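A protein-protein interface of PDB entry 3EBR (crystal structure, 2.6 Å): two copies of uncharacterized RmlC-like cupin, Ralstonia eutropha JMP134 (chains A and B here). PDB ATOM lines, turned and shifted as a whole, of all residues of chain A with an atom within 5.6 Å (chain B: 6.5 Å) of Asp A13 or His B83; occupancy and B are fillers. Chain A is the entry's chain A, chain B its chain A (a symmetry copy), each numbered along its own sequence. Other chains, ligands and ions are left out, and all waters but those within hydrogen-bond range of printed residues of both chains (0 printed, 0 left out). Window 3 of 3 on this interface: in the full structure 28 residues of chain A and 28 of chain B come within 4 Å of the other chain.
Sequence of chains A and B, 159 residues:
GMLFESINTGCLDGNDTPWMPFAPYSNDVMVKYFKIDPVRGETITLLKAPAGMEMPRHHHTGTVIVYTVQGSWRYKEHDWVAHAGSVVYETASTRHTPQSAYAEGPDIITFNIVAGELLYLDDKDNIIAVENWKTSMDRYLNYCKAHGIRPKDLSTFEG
Of the 8 printed residues of chain A, 5 touch a printed residue of chain B.
Hydrophobic or aromatic side chains of chain A that line the printed part of chain B: Phe A34.
Hydrophobic or aromatic side chains of chain B within 4 Å of the printed part of chain A: His B83 and Val B87.
Among the printed residues, 9 pairs touch across the chains.
Among the printed residues, no Asp or Glu carboxylate lies within 4 Å of a Lys or Arg side-chain nitrogen of the other chain.
Among the printed residues, merely in contact across the chains: Cys A11 with Val B87 (3.5 Å), Leu A12 with Ser B86 (3.5 Å), Asp A13 with Ser B86 (3.7 Å), Gly A14 with Gly B85 (3.4 Å), Gly A14 with Ser B86 (3.9 Å), Phe A34 with Gly B85 (3.4 Å) and Phe A34 with Val B87 (3.4 Å).
A ring nitrogen (ND1) of His B83 sits at hydrogen-bond distance from the side-chain carboxylate (OD1) of Asp A13 (2.9 Å).
The backbone NH (N) of Leu A12 sits at hydrogen-bond distance from the backbone carbonyl oxygen (O) of Val B87.
The side-chain carboxylate (OD2) of Asp A13 lies close to the side-chain amide oxygen (OD1) of Asn A15.
The backbone carbonyl oxygen (O) of Thr B68 sits at hydrogen-bond distance from the backbone NH (N) of Gly B85.
N of Thr B68 lies within hydrogen-bond range of O of Ser B86, at 3.3 Å.
OG of Ser B86 lies within hydrogen-bond range of O of His B83 (2.5 Å).
O of Val B81 lies within hydrogen-bond range of ND1 of His B83 (3.4 Å).
No position is printed for both chains.
Of the 9 pairs that touch across the chains among the printed residues, none has its exchanged pair printed and touching as well.
Of chain B, only His B83 (2.9 Å) and Ser B86 (3.7 Å) come within 4 Å of Asp A13.
His B83 touches just one residue of chain A: Asp A13.
Of the printed residues of chain A, Val B87 touches Cys A11, Leu A12 and Phe A34.
Printed residues of chain A within 4 Å of Gly B85: Gly A14 and Phe A34.
Of the printed residues of chain B, Gly A14 touches Gly B85 (3.4 Å) and Ser B86 (3.9 Å).
Of the printed residues of chain B, Leu A12 touches Ser B86 (3.5 Å) and Val B87 (3.1 Å).
Tyr B67 touches none of the printed residues of chain A.
The nearest printed residue of chain A that does not touch His B83 is Cys A11 (5.6 Å).
The nearest printed residue of chain A that does not touch Ser B86 is Phe A34 (4.4 Å).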
ATOM      1  N   CYS A  11       8.747  -0.017  31.837  1.00  0.00           N
ATOM      2  CA  CYS A  11       8.894  -0.934  30.729  1.00  0.00           C
ATOM      3  C   CYS A  11       8.360  -2.292  31.122  1.00  0.00           C
ATOM      4  O   CYS A  11       8.786  -2.823  32.143  1.00  0.00           O
ATOM      5  CB  CYS A  11      10.365  -1.071  30.370  1.00  0.00           C
ATOM      6  SG  CYS A  11      10.676  -2.289  29.090  1.00  0.00           S
ATOM      7  N   LEU A  12       7.433  -2.830  30.326  1.00  0.00           N
ATOM      8  CA  LEU A  12       6.837  -4.145  30.551  1.00  0.00           C
ATOM      9  C   LEU A  12       7.235  -4.981  29.349  1.00  0.00           C
ATOM     10  O   LEU A  12       6.831  -4.675  28.218  1.00  0.00           O
ATOM     11  CB  LEU A  12       5.322  -4.038  30.713  1.00  0.00           C
ATOM     12  CG  LEU A  12       4.518  -5.293  31.054  1.00  0.00           C
ATOM     13  CD1 LEU A  12       5.032  -6.007  32.303  1.00  0.00           C
ATOM     14  CD2 LEU A  12       3.061  -4.899  31.230  1.00  0.00           C
ATOM     15  N   ASP A  13       8.042  -6.018  29.593  1.00  0.00           N
ATOM     16  CA  ASP A  13       8.542  -6.884  28.530  1.00  0.00           C
ATOM     17  C   ASP A  13       7.407  -7.798  28.051  1.00  0.00           C
ATOM     18  O   ASP A  13       6.457  -8.059  28.795  1.00  0.00           O
ATOM     19  CB  ASP A  13       9.751  -7.702  29.014  1.00  0.00           C
ATOM     20  CG  ASP A  13      10.666  -8.120  27.876  1.00  0.00           C
ATOM     21  OD1 ASP A  13      11.293  -7.219  27.263  1.00  0.00           O
ATOM     22  OD2 ASP A  13      10.826  -9.333  27.649  1.00  0.00           O
ATOM     23  N   GLY A  14       7.503  -8.253  26.804  1.00  0.00           N
ATOM     24  CA  GLY A  14       6.497  -9.132  26.194  1.00  0.00           C
ATOM     25  C   GLY A  14       6.095 -10.372  26.986  1.00  0.00           C
ATOM     26  O   GLY A  14       4.917 -10.714  27.033  1.00  0.00           O
ATOM     27  N   ASN A  15       7.068 -10.998  27.646  1.00  0.00           N
ATOM     28  CA  ASN A  15       6.821 -12.209  28.470  1.00  0.00           C
ATOM     29  C   ASN A  15       6.736 -11.916  30.015  1.00  0.00           C
ATOM     30  O   ASN A  15       7.050 -12.790  30.820  1.00  0.00           O
ATOM     31  CB  ASN A  15       7.750 -13.407  28.043  1.00  0.00           C
ATOM     32  CG  ASN A  15       9.200 -13.027  27.858  1.00  0.00           C
ATOM     33  OD1 ASN A  15       9.645 -11.987  28.326  1.00  0.00           O
ATOM     34  ND2 ASN A  15       9.935 -13.861  27.140  1.00  0.00           N
ATOM     35  N   ASP A  16       6.332 -10.692  30.390  1.00  0.00           N
ATOM     36  CA  ASP A  16       6.067 -10.273  31.794  1.00  0.00           C
ATOM     37  C   ASP A  16       4.564  -9.913  32.001  1.00  0.00           C
ATOM     38  O   ASP A  16       4.172  -9.396  33.058  1.00  0.00           O
ATOM     39  CB  ASP A  16       6.980  -9.116  32.226  1.00  0.00           C
ATOM     40  CG  ASP A  16       8.442  -9.519  32.361  1.00  0.00           C
ATOM     41  OD1 ASP A  16       8.778 -10.724  32.460  1.00  0.00           O
ATOM     42  OD2 ASP A  16       9.270  -8.591  32.410  1.00  0.00           O
ATOM     43  N   THR A  17       3.744 -10.198  30.985  1.00  0.00           N
ATOM     44  CA  THR A  17       2.312  -9.991  30.974  1.00  0.00           C
ATOM     45  C   THR A  17       1.810 -11.161  30.095  1.00  0.00           C
ATOM     46  O   THR A  17       2.300 -11.334  28.972  1.00  0.00           O
ATOM     47  CB  THR A  17       1.920  -8.596  30.474  1.00  0.00           C
ATOM     48  OG1 THR A  17       0.494  -8.530  30.388  1.00  0.00           O
ATOM     49  CG2 THR A  17       2.529  -8.283  29.113  1.00  0.00           C
ATOM     50  N   PHE A  34      -0.726  -4.386  28.433  1.00  0.00           N
ATOM     51  CA  PHE A  34       0.493  -3.647  28.801  1.00  0.00           C
ATOM     52  C   PHE A  34       0.204  -2.470  29.727  1.00  0.00           C
ATOM     53  O   PHE A  34       1.006  -2.193  30.611  1.00  0.00           O
ATOM     54  CB  PHE A  34       1.237  -3.150  27.560  1.00  0.00           C
ATOM     55  CG  PHE A  34       1.891  -4.247  26.778  1.00  0.00           C
ATOM     56  CD1 PHE A  34       3.184  -4.652  27.086  1.00  0.00           C
ATOM     57  CD2 PHE A  34       1.218  -4.888  25.754  1.00  0.00           C
ATOM     58  CE1 PHE A  34       3.803  -5.665  26.377  1.00  0.00           C
ATOM     59  CE2 PHE A  34       1.832  -5.910  25.038  1.00  0.00           C
ATOM     60  CZ  PHE A  34       3.129  -6.297  25.350  1.00  0.00           C
ATOM     61  N   TYR B  67       6.709   0.896  21.297  1.00  0.00           N
ATOM     62  CA  TYR B  67       6.538  -0.530  21.068  1.00  0.00           C
ATOM     63  C   TYR B  67       7.748  -0.952  20.215  1.00  0.00           C
ATOM     64  O   TYR B  67       7.924  -0.454  19.100  1.00  0.00           O
ATOM     65  CB  TYR B  67       5.237  -0.876  20.361  1.00  0.00           C
ATOM     66  CG  TYR B  67       5.185  -2.338  19.977  1.00  0.00           C
ATOM     67  CD1 TYR B  67       4.979  -3.316  20.940  1.00  0.00           C
ATOM     68  CD2 TYR B  67       5.373  -2.744  18.656  1.00  0.00           C
ATOM     69  CE1 TYR B  67       4.952  -4.677  20.599  1.00  0.00           C
ATOM     70  CE2 TYR B  67       5.355  -4.102  18.306  1.00  0.00           C
ATOM     71  CZ  TYR B  67       5.133  -5.056  19.282  1.00  0.00           C
ATOM     72  OH  TYR B  67       5.102  -6.378  18.938  1.00  0.00           O
ATOM     73  N   THR B  68       8.547  -1.884  20.723  1.00  0.00           N
ATOM     74  CA  THR B  68       9.747  -2.357  20.033  1.00  0.00           C
ATOM     75  C   THR B  68       9.377  -3.453  19.040  1.00  0.00           C
ATOM     76  O   THR B  68       8.969  -4.551  19.437  1.00  0.00           O
ATOM     77  CB  THR B  68      10.767  -2.866  21.052  1.00  0.00           C
ATOM     78  OG1 THR B  68      10.998  -1.831  22.015  1.00  0.00           O
ATOM     79  CG2 THR B  68      12.081  -3.272  20.376  1.00  0.00           C
ATOM     80  N   VAL B  69       9.519  -3.143  17.751  1.00  0.00           N
ATOM     81  CA  VAL B  69       9.178  -4.080  16.671  1.00  0.00           C
ATOM     82  C   VAL B  69      10.289  -5.128  16.608  1.00  0.00           C
ATOM     83  O   VAL B  69       9.997  -6.324  16.528  1.00  0.00           O
ATOM     84  CB  VAL B  69       8.931  -3.351  15.343  1.00  0.00           C
ATOM     85  CG1 VAL B  69       8.560  -4.331  14.261  1.00  0.00           C
ATOM     86  CG2 VAL B  69       7.805  -2.341  15.518  1.00  0.00           C
ATOM     87  N   GLN B  70      11.547  -4.680  16.626  1.00  0.00           N
ATOM     88  CA  GLN B  70      12.692  -5.599  16.674  1.00  0.00           C
ATOM     89  C   GLN B  70      13.902  -4.925  17.290  1.00  0.00           C
ATOM     90  O   GLN B  70      13.977  -3.695  17.347  1.00  0.00           O
ATOM     91  CB  GLN B  70      13.079  -6.182  15.311  1.00  0.00           C
ATOM     92  CG  GLN B  70      13.623  -5.219  14.270  1.00  0.00           C
ATOM     93  CD  GLN B  70      14.398  -5.957  13.189  1.00  0.00           C
ATOM     94  OE1 GLN B  70      13.963  -6.997  12.695  1.00  0.00           O
ATOM     95  NE2 GLN B  70      15.553  -5.417  12.819  1.00  0.00           N
ATOM     96  N   GLY B  71      14.853  -5.762  17.698  1.00  0.00           N
ATOM     97  CA  GLY B  71      16.081  -5.329  18.327  1.00  0.00           C
ATOM     98  C   GLY B  71      15.872  -5.081  19.803  1.00  0.00           C
ATOM     99  O   GLY B  71      14.772  -5.300  20.329  1.00  0.00           O
ATOM    100  N   SER B  72      16.944  -4.663  20.478  1.00  0.00           N
ATOM    101  CA  SER B  72      16.905  -4.356  21.911  1.00  0.00           C
ATOM    102  C   SER B  72      17.606  -3.037  22.174  1.00  0.00           C
ATOM    103  O   SER B  72      18.602  -2.723  21.525  1.00  0.00           O
ATOM    104  CB  SER B  72      17.542  -5.459  22.751  1.00  0.00           C
ATOM    105  OG  SER B  72      16.978  -6.716  22.449  1.00  0.00           O
ATOM    106  N   TRP B  73      17.081  -2.277  23.127  1.00  0.00           N
ATOM    107  CA  TRP B  73      17.641  -0.982  23.492  1.00  0.00           C
ATOM    108  C   TRP B  73      17.312  -0.691  24.944  1.00  0.00           C
ATOM    109  O   TRP B  73      16.593  -1.454  25.594  1.00  0.00           O
ATOM    110  CB  TRP B  73      17.112   0.105  22.553  1.00  0.00           C
ATOM    111  CG  TRP B  73      15.638   0.256  22.601  1.00  0.00           C
ATOM    112  CD1 TRP B  73      14.728  -0.422  21.861  1.00  0.00           C
ATOM    113  CD2 TRP B  73      14.895   1.143  23.442  1.00  0.00           C
ATOM    114  NE1 TRP B  73      13.467  -0.023  22.192  1.00  0.00           N
ATOM    115  CE2 TRP B  73      13.534   0.938  23.161  1.00  0.00           C
ATOM    116  CE3 TRP B  73      15.252   2.085  24.410  1.00  0.00           C
ATOM    117  CZ2 TRP B  73      12.520   1.648  23.809  1.00  0.00           C
ATOM    118  CZ3 TRP B  73      14.259   2.780  25.057  1.00  0.00           C
ATOM    119  CH2 TRP B  73      12.903   2.564  24.757  1.00  0.00           C
ATOM    120  N   VAL B  81      16.052  -3.342  30.063  1.00  0.00           N
ATOM    121  CA  VAL B  81      16.278  -3.391  28.615  1.00  0.00           C
ATOM    122  C   VAL B  81      14.956  -3.712  27.926  1.00  0.00           C
ATOM    123  O   VAL B  81      14.271  -4.653  28.334  1.00  0.00           O
ATOM    124  CB  VAL B  81      17.307  -4.450  28.213  1.00  0.00           C
ATOM    125  CG1 VAL B  81      17.473  -4.495  26.694  1.00  0.00           C
ATOM    126  CG2 VAL B  81      18.635  -4.159  28.867  1.00  0.00           C
ATOM    127  N   ALA B  82      14.597  -2.915  26.916  1.00  0.00           N
ATOM    128  CA  ALA B  82      13.379  -3.104  26.147  1.00  0.00           C
ATOM    129  C   ALA B  82      13.709  -4.032  24.997  1.00  0.00           C
ATOM    130  O   ALA B  82      14.561  -3.686  24.184  1.00  0.00           O
ATOM    131  CB  ALA B  82      12.850  -1.776  25.615  1.00  0.00           C
ATOM    132  N   HIS B  83      13.069  -5.205  24.952  1.00  0.00           N
ATOM    133  CA  HIS B  83      13.258  -6.196  23.877  1.00  0.00           C
ATOM    134  C   HIS B  83      12.098  -6.109  22.905  1.00  0.00           C
ATOM    135  O   HIS B  83      11.144  -5.382  23.163  1.00  0.00           O
ATOM    136  CB  HIS B  83      13.308  -7.608  24.446  1.00  0.00           C
ATOM    137  CG  HIS B  83      14.371  -7.796  25.474  1.00  0.00           C
ATOM    138  ND1 HIS B  83      14.126  -7.665  26.824  1.00  0.00           N
ATOM    139  CD2 HIS B  83      15.691  -8.071  25.352  1.00  0.00           C
ATOM    140  CE1 HIS B  83      15.246  -7.870  27.493  1.00  0.00           C
ATOM    141  NE2 HIS B  83      16.209  -8.126  26.623  1.00  0.00           N
ATOM    142  N   ALA B  84      12.187  -6.845  21.794  1.00  0.00           N
ATOM    143  CA  ALA B  84      11.123  -6.902  20.788  1.00  0.00           C
ATOM    144  C   ALA B  84       9.876  -7.462  21.470  1.00  0.00           C
ATOM    145  O   ALA B  84       9.978  -8.423  22.235  1.00  0.00           O
ATOM    146  CB  ALA B  84      11.519  -7.762  19.619  1.00  0.00           C
ATOM    147  N   GLY B  85       8.729  -6.826  21.239  1.00  0.00           N
ATOM    148  CA  GLY B  85       7.461  -7.213  21.868  1.00  0.00           C
ATOM    149  C   GLY B  85       7.158  -6.494  23.181  1.00  0.00           C
ATOM    150  O   GLY B  85       6.096  -6.723  23.769  1.00  0.00           O
ATOM    151  N   SER B  86       8.066  -5.624  23.643  1.00  0.00           N
ATOM    152  CA  SER B  86       7.881  -4.871  24.878  1.00  0.00           C
ATOM    153  C   SER B  86       7.238  -3.532  24.576  1.00  0.00           C
ATOM    154  O   SER B  86       7.166  -3.120  23.416  1.00  0.00           O
ATOM    155  CB  SER B  86       9.217  -4.622  25.571  1.00  0.00           C
ATOM    156  OG  SER B  86      10.052  -3.794  24.791  1.00  0.00           O
ATOM    157  N   VAL B  87       6.765  -2.888  25.644  1.00  0.00           N
ATOM    158  CA  VAL B  87       6.148  -1.570  25.609  1.00  0.00           C
ATOM    159  C   VAL B  87       6.804  -0.708  26.682  1.00  0.00           C
ATOM    160  O   VAL B  87       6.856  -1.125  27.838  1.00  0.00           O
ATOM    161  CB  VAL B  87       4.620  -1.592  25.855  1.00  0.00           C
ATOM    162  CG1 VAL B  87       4.062  -0.158  25.963  1.00  0.00           C
ATOM    163  CG2 VAL B  87       3.924  -2.330  24.760  1.00  0.00           C
ATOM    164  N   ALA B 101      21.172  -1.917  23.168  1.00  0.00           N
ATOM    165  CA  ALA B 101      21.482  -2.879  24.240  1.00  0.00           C
ATOM    166  C   ALA B 101      22.688  -3.777  23.935  1.00  0.00           C
ATOM    167  O   ALA B 101      23.069  -4.560  24.795  1.00  0.00           O
ATOM    168  CB  ALA B 101      20.260  -3.756  24.539  1.00  0.00           C
